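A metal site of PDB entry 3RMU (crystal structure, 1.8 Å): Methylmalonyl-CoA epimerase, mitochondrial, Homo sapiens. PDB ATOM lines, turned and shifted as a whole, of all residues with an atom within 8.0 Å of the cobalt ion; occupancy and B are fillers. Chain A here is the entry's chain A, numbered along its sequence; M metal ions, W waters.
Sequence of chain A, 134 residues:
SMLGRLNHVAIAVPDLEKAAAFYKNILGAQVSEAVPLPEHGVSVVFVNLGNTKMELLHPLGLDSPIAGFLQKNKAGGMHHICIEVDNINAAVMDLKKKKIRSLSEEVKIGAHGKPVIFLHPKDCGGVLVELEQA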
ATOM      1  N   ASN A   7      13.503  22.033  10.712  1.00  0.00           N
ATOM      2  CA  ASN A   7      14.896  22.459  10.789  1.00  0.00           C
ATOM      3  C   ASN A   7      15.429  22.931   9.412  1.00  0.00           C
ATOM      4  O   ASN A   7      15.978  23.995   9.300  1.00  0.00           O
ATOM      5  CB  ASN A   7      15.727  21.346  11.407  1.00  0.00           C
ATOM      6  CG  ASN A   7      17.158  21.713  11.542  1.00  0.00           C
ATOM      7  OD1 ASN A   7      17.923  21.728  10.570  1.00  0.00           O
ATOM      8  ND2 ASN A   7      17.554  22.006  12.775  1.00  0.00           N
ATOM      9  N   HIS A   8      15.231  22.145   8.361  1.00  0.00           N
ATOM     10  CA  HIS A   8      15.650  22.563   7.028  1.00  0.00           C
ATOM     11  C   HIS A   8      14.871  21.863   5.940  1.00  0.00           C
ATOM     12  O   HIS A   8      14.270  20.797   6.187  1.00  0.00           O
ATOM     13  CB  HIS A   8      17.177  22.353   6.795  1.00  0.00           C
ATOM     14  CG  HIS A   8      17.697  20.935   6.983  1.00  0.00           C
ATOM     15  ND1 HIS A   8      18.211  20.501   8.177  1.00  0.00           N
ATOM     16  CD2 HIS A   8      17.942  19.946   6.081  1.00  0.00           C
ATOM     17  CE1 HIS A   8      18.661  19.251   8.031  1.00  0.00           C
ATOM     18  NE2 HIS A   8      18.493  18.885   6.767  1.00  0.00           N
ATOM     19  N   VAL A   9      14.872  22.493   4.774  1.00  0.00           N
ATOM     20  CA  VAL A   9      14.488  21.834   3.521  1.00  0.00           C
ATOM     21  C   VAL A   9      15.792  21.691   2.794  1.00  0.00           C
ATOM     22  O   VAL A   9      16.525  22.666   2.671  1.00  0.00           O
ATOM     23  CB  VAL A   9      13.478  22.636   2.708  1.00  0.00           C
ATOM     24  CG1 VAL A   9      13.260  21.969   1.350  1.00  0.00           C
ATOM     25  CG2 VAL A   9      12.190  22.677   3.411  1.00  0.00           C
ATOM     26  N   ALA A  10      16.127  20.490   2.334  1.00  0.00           N
ATOM     27  CA  ALA A  10      17.408  20.230   1.640  1.00  0.00           C
ATOM     28  C   ALA A  10      17.136  20.192   0.134  1.00  0.00           C
ATOM     29  O   ALA A  10      16.232  19.497  -0.312  1.00  0.00           O
ATOM     30  CB  ALA A  10      17.996  18.845   1.994  1.00  0.00           C
ATOM     31  N   ILE A  11      17.922  20.952  -0.608  1.00  0.00           N
ATOM     32  CA  ILE A  11      17.849  21.001  -2.090  1.00  0.00           C
ATOM     33  C   ILE A  11      19.175  20.558  -2.649  1.00  0.00           C
ATOM     34  O   ILE A  11      20.213  21.117  -2.283  1.00  0.00           O
ATOM     35  CB  ILE A  11      17.571  22.459  -2.624  1.00  0.00           C
ATOM     36  CG1 ILE A  11      16.396  23.146  -1.910  1.00  0.00           C
ATOM     37  CG2 ILE A  11      17.407  22.453  -4.183  1.00  0.00           C
ATOM     38  CD1 ILE A  11      15.110  22.463  -1.932  1.00  0.00           C
ATOM     39  N   GLU A  55      19.024  24.038   2.941  1.00  0.00           N
ATOM     40  CA  GLU A  55      20.410  23.537   2.871  1.00  0.00           C
ATOM     41  C   GLU A  55      20.570  23.176   1.414  1.00  0.00           C
ATOM     42  O   GLU A  55      19.919  22.247   0.918  1.00  0.00           O
ATOM     43  CB  GLU A  55      20.666  22.329   3.754  1.00  0.00           C
ATOM     44  CG  GLU A  55      20.516  22.689   5.274  1.00  0.00           C
ATOM     45  CD  GLU A  55      21.075  21.639   6.235  1.00  0.00           C
ATOM     46  OE1 GLU A  55      21.611  20.606   5.766  1.00  0.00           O
ATOM     47  OE2 GLU A  55      20.956  21.894   7.475  1.00  0.00           O
ATOM     48  N   LEU A  57      22.812  21.536  -1.371  1.00  0.00           N
ATOM     49  CA  LEU A  57      23.741  20.434  -1.199  1.00  0.00           C
ATOM     50  C   LEU A  57      24.318  20.079  -2.546  1.00  0.00           C
ATOM     51  O   LEU A  57      23.580  20.069  -3.523  1.00  0.00           O
ATOM     52  CB  LEU A  57      23.013  19.194  -0.675  1.00  0.00           C
ATOM     53  CG  LEU A  57      22.372  19.331   0.714  1.00  0.00           C
ATOM     54  CD1 LEU A  57      21.634  18.006   1.076  1.00  0.00           C
ATOM     55  CD2 LEU A  57      23.424  19.686   1.734  1.00  0.00           C
ATOM     56  N   HIS A  79      15.357  17.450  -1.991  1.00  0.00           N
ATOM     57  CA  HIS A  79      15.880  16.132  -1.653  1.00  0.00           C
ATOM     58  C   HIS A  79      15.247  15.602  -0.352  1.00  0.00           C
ATOM     59  O   HIS A  79      14.856  14.443  -0.296  1.00  0.00           O
ATOM     60  CB  HIS A  79      17.407  16.165  -1.543  1.00  0.00           C
ATOM     61  CG  HIS A  79      17.997  14.834  -1.278  1.00  0.00           C
ATOM     62  ND1 HIS A  79      18.360  14.407  -0.024  1.00  0.00           N
ATOM     63  CD2 HIS A  79      18.304  13.813  -2.115  1.00  0.00           C
ATOM     64  CE1 HIS A  79      18.818  13.174  -0.083  1.00  0.00           C
ATOM     65  NE2 HIS A  79      18.794  12.787  -1.348  1.00  0.00           N
ATOM     66  N   HIS A  80      15.169  16.406   0.719  1.00  0.00           N
ATOM     67  CA  HIS A  80      14.517  15.941   1.960  1.00  0.00           C
ATOM     68  C   HIS A  80      14.007  17.109   2.790  1.00  0.00           C
ATOM     69  O   HIS A  80      14.388  18.241   2.544  1.00  0.00           O
ATOM     70  CB  HIS A  80      15.418  15.009   2.834  1.00  0.00           C
ATOM     71  CG  HIS A  80      16.661  15.630   3.416  1.00  0.00           C
ATOM     72  ND1 HIS A  80      17.885  15.589   2.783  1.00  0.00           N
ATOM     73  CD2 HIS A  80      16.890  16.217   4.624  1.00  0.00           C
ATOM     74  CE1 HIS A  80      18.795  16.151   3.559  1.00  0.00           C
ATOM     75  NE2 HIS A  80      18.227  16.542   4.685  1.00  0.00           N
ATOM     76  N   ILE A  81      13.168  16.814   3.762  1.00  0.00           N
ATOM     77  CA  ILE A  81      12.835  17.789   4.817  1.00  0.00           C
ATOM     78  C   ILE A  81      13.357  17.252   6.135  1.00  0.00           C
ATOM     79  O   ILE A  81      13.379  16.034   6.357  1.00  0.00           O
ATOM     80  CB  ILE A  81      11.330  18.044   4.870  1.00  0.00           C
ATOM     81  CG1 ILE A  81      10.524  16.749   5.046  1.00  0.00           C
ATOM     82  CG2 ILE A  81      10.878  18.771   3.556  1.00  0.00           C
ATOM     83  CD1 ILE A  81       9.008  16.977   5.317  1.00  0.00           C
ATOM     84  N   CYS A  82      13.765  18.139   7.028  1.00  0.00           N
ATOM     85  CA  CYS A  82      14.249  17.699   8.286  1.00  0.00           C
ATOM     86  C   CYS A  82      13.403  18.295   9.382  1.00  0.00           C
ATOM     87  O   CYS A  82      13.276  19.506   9.491  1.00  0.00           O
ATOM     88  CB  CYS A  82      15.711  18.063   8.487  1.00  0.00           C
ATOM     89  SG  CYS A  82      16.318  17.702  10.153  1.00  0.00           S
ATOM     90  N   ILE A  83      12.798  17.412  10.175  1.00  0.00           N
ATOM     91  CA  ILE A  83      11.945  17.826  11.279  1.00  0.00           C
ATOM     92  C   ILE A  83      12.570  17.423  12.631  1.00  0.00           C
ATOM     93  O   ILE A  83      13.093  16.304  12.813  1.00  0.00           O
ATOM     94  CB  ILE A  83      10.490  17.260  11.137  1.00  0.00           C
ATOM     95  CG1 ILE A  83       9.918  17.542   9.752  1.00  0.00           C
ATOM     96  CG2 ILE A  83       9.528  17.823  12.237  1.00  0.00           C
ATOM     97  CD1 ILE A  83       8.534  16.906   9.529  1.00  0.00           C
ATOM     98  N   GLY A 110      24.296  13.158  12.145  1.00  0.00           N
ATOM     99  CA  GLY A 110      24.194  14.005  10.939  1.00  0.00           C
ATOM    100  C   GLY A 110      25.129  15.213  10.945  1.00  0.00           C
ATOM    101  O   GLY A 110      25.937  15.384  11.871  1.00  0.00           O
ATOM    102  N   ALA A 111      25.008  16.079   9.933  1.00  0.00           N
ATOM    103  CA  ALA A 111      26.000  17.169   9.732  1.00  0.00           C
ATOM    104  C   ALA A 111      25.995  18.207  10.847  1.00  0.00           C
ATOM    105  O   ALA A 111      26.984  18.942  11.035  1.00  0.00           O
ATOM    106  CB  ALA A 111      25.806  17.846   8.419  1.00  0.00           C
ATOM    107  N   HIS A 112      24.888  18.272  11.606  1.00  0.00           N
ATOM    108  CA  HIS A 112      24.766  19.231  12.697  1.00  0.00           C
ATOM    109  C   HIS A 112      25.387  18.709  13.998  1.00  0.00           C
ATOM    110  O   HIS A 112      25.371  19.388  15.026  1.00  0.00           O
ATOM    111  CB  HIS A 112      23.298  19.617  12.906  1.00  0.00           C
ATOM    112  CG  HIS A 112      22.587  20.045  11.654  1.00  0.00           C
ATOM    113  ND1 HIS A 112      21.233  19.904  11.497  1.00  0.00           N
ATOM    114  CD2 HIS A 112      23.049  20.584  10.495  1.00  0.00           C
ATOM    115  CE1 HIS A 112      20.883  20.354  10.301  1.00  0.00           C
ATOM    116  NE2 HIS A 112      21.960  20.770   9.676  1.00  0.00           N
ATOM    117  N   VAL A 116      20.428  11.496  13.944  1.00  0.00           N
ATOM    118  CA  VAL A 116      19.319  11.575  12.991  1.00  0.00           C
ATOM    119  C   VAL A 116      18.906  10.217  12.510  1.00  0.00           C
ATOM    120  O   VAL A 116      19.685   9.273  12.571  1.00  0.00           O
ATOM    121  CB  VAL A 116      19.688  12.377  11.674  1.00  0.00           C
ATOM    122  CG1 VAL A 116      20.105  13.823  12.006  1.00  0.00           C
ATOM    123  CG2 VAL A 116      20.799  11.647  10.938  1.00  0.00           C
ATOM    124  N   PHE A 118      16.318   8.599   9.045  1.00  0.00           N
ATOM    125  CA  PHE A 118      15.559   8.936   7.855  1.00  0.00           C
ATOM    126  C   PHE A 118      14.377   7.974   7.682  1.00  0.00           C
ATOM    127  O   PHE A 118      14.487   6.770   7.962  1.00  0.00           O
ATOM    128  CB  PHE A 118      16.476   8.907   6.616  1.00  0.00           C
ATOM    129  CG  PHE A 118      17.426  10.085   6.520  1.00  0.00           C
ATOM    130  CD1 PHE A 118      17.097  11.206   5.756  1.00  0.00           C
ATOM    131  CD2 PHE A 118      18.643  10.071   7.199  1.00  0.00           C
ATOM    132  CE1 PHE A 118      17.997  12.293   5.637  1.00  0.00           C
ATOM    133  CE2 PHE A 118      19.541  11.175   7.104  1.00  0.00           C
ATOM    134  CZ  PHE A 118      19.204  12.282   6.325  1.00  0.00           C
ATOM    135  N   LEU A 128      11.176  12.168   1.387  1.00  0.00           N
ATOM    136  CA  LEU A 128      12.221  11.702   2.330  1.00  0.00           C
ATOM    137  C   LEU A 128      12.270  12.611   3.542  1.00  0.00           C
ATOM    138  O   LEU A 128      12.511  13.810   3.412  1.00  0.00           O
ATOM    139  CB  LEU A 128      13.588  11.594   1.669  1.00  0.00           C
ATOM    140  CG  LEU A 128      14.786  11.266   2.572  1.00  0.00           C
ATOM    141  CD1 LEU A 128      14.698   9.851   3.138  1.00  0.00           C
ATOM    142  CD2 LEU A 128      16.085  11.392   1.787  1.00  0.00           C
ATOM    143  N   VAL A 129      12.043  12.031   4.708  1.00  0.00           N
ATOM    144  CA  VAL A 129      11.972  12.791   5.946  1.00  0.00           C
ATOM    145  C   VAL A 129      13.136  12.406   6.863  1.00  0.00           C
ATOM    146  O   VAL A 129      13.346  11.227   7.155  1.00  0.00           O
ATOM    147  CB  VAL A 129      10.661  12.610   6.683  1.00  0.00           C
ATOM    148  CG1 VAL A 129      10.690  13.371   8.024  1.00  0.00           C
ATOM    149  CG2 VAL A 129       9.447  13.035   5.795  1.00  0.00           C
ATOM    150  N   GLU A 130      13.898  13.417   7.282  1.00  0.00           N
ATOM    151  CA  GLU A 130      15.010  13.238   8.258  1.00  0.00           C
ATOM    152  C   GLU A 130      14.436  13.742   9.573  1.00  0.00           C
ATOM    153  O   GLU A 130      13.789  14.786   9.608  1.00  0.00           O
ATOM    154  CB  GLU A 130      16.170  14.130   7.802  1.00  0.00           C
ATOM    155  CG  GLU A 130      17.355  14.283   8.741  1.00  0.00           C
ATOM    156  CD  GLU A 130      18.461  15.200   8.190  1.00  0.00           C
ATOM    157  OE1 GLU A 130      18.318  16.070   7.248  1.00  0.00           O
ATOM    158  OE2 GLU A 130      19.568  14.999   8.749  1.00  0.00           O
ATOM    159  N   LEU A 131      14.578  12.959  10.613  1.00  0.00           N
ATOM    160  CA  LEU A 131      14.202  13.358  11.978  1.00  0.00           C
ATOM    161  C   LEU A 131      15.480  13.580  12.763  1.00  0.00           C
ATOM    162  O   LEU A 131      16.387  12.762  12.729  1.00  0.00           O
ATOM    163  CB  LEU A 131      13.360  12.308  12.679  1.00  0.00           C
ATOM    164  CG  LEU A 131      11.976  12.028  12.052  1.00  0.00           C
ATOM    165  CD1 LEU A 131      11.258  10.895  12.784  1.00  0.00           C
ATOM    166  CD2 LEU A 131      11.136  13.329  12.027  1.00  0.00           C
ATOM    167  N   GLU A 132      15.537  14.701  13.478  1.00  0.00           N
ATOM    168  CA  GLU A 132      16.767  15.094  14.149  1.00  0.00           C
ATOM    169  C   GLU A 132      16.471  15.519  15.538  1.00  0.00           C
ATOM    170  O   GLU A 132      15.508  16.226  15.808  1.00  0.00           O
ATOM    171  CB  GLU A 132      17.479  16.210  13.344  1.00  0.00           C
ATOM    172  CG  GLU A 132      18.738  16.737  14.056  1.00  0.00           C
ATOM    173  CD  GLU A 132      19.556  17.731  13.221  1.00  0.00           C
ATOM    174  OE1 GLU A 132      20.428  17.310  12.433  1.00  0.00           O
ATOM    175  OE2 GLU A 132      19.321  18.930  13.357  1.00  0.00           O
HETATM  176 CO    CO M   1      19.349  17.175   6.163  1.00  0.00          CO
HETATM  177  O   HOH W   1      21.177  15.746   6.047  1.00  0.00           O
HETATM  178  O   HOH W   2      20.721  18.350   4.679  1.00  0.00           O
HETATM  179  O   HOH W   3      21.346  17.570   7.361  1.00  0.00           O
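Of the 22 residues printed, 3 come within 4 Å of the cobalt ion. The nearest printed residue that does not touch the cobalt ion is Glu 55 (4.1 Å).
The backbone NH (N) of Glu 130 is in hydrogen-bond range of the backbone carbonyl oxygen (O) of Ile 81 (2.8 Å). The backbone NH (N) of Ile 83 sits at hydrogen-bond distance from the backbone carbonyl oxygen (O) of Glu 130 (2.9 Å). N of Ala 10 is in hydrogen-bond range of O of His 80 (2.9 Å). ND1 of His 80 lies within hydrogen-bond range of ND1 of His 79, 3.1 Å away. A ring nitrogen (ND1) of His 8 lies within hydrogen-bond range of the side-chain carboxylate (OE2) of Glu 55 (3.2 Å). O of His 8 lies within hydrogen-bond range of N of Cys 82, 2.8 Å away. ND1 of His 8 lies within hydrogen-bond range of OD1 of Asn 7 (2.7 Å).
Water W3 bridges OE2 of Glu 130 (3.4 Å) and OE1 of Glu 55 (3.4 Å).
The cobalt ion is bound by the side-chain carboxylate of Glu 130 (1.9 Å), a ring nitrogen (NE2) of His 80 (2.0 Å), a ring nitrogen (NE2) of His 8 (2.0 Å), water W1 (2.3 Å), water W2 (2.3 Å) and water W3 (2.4 Å).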
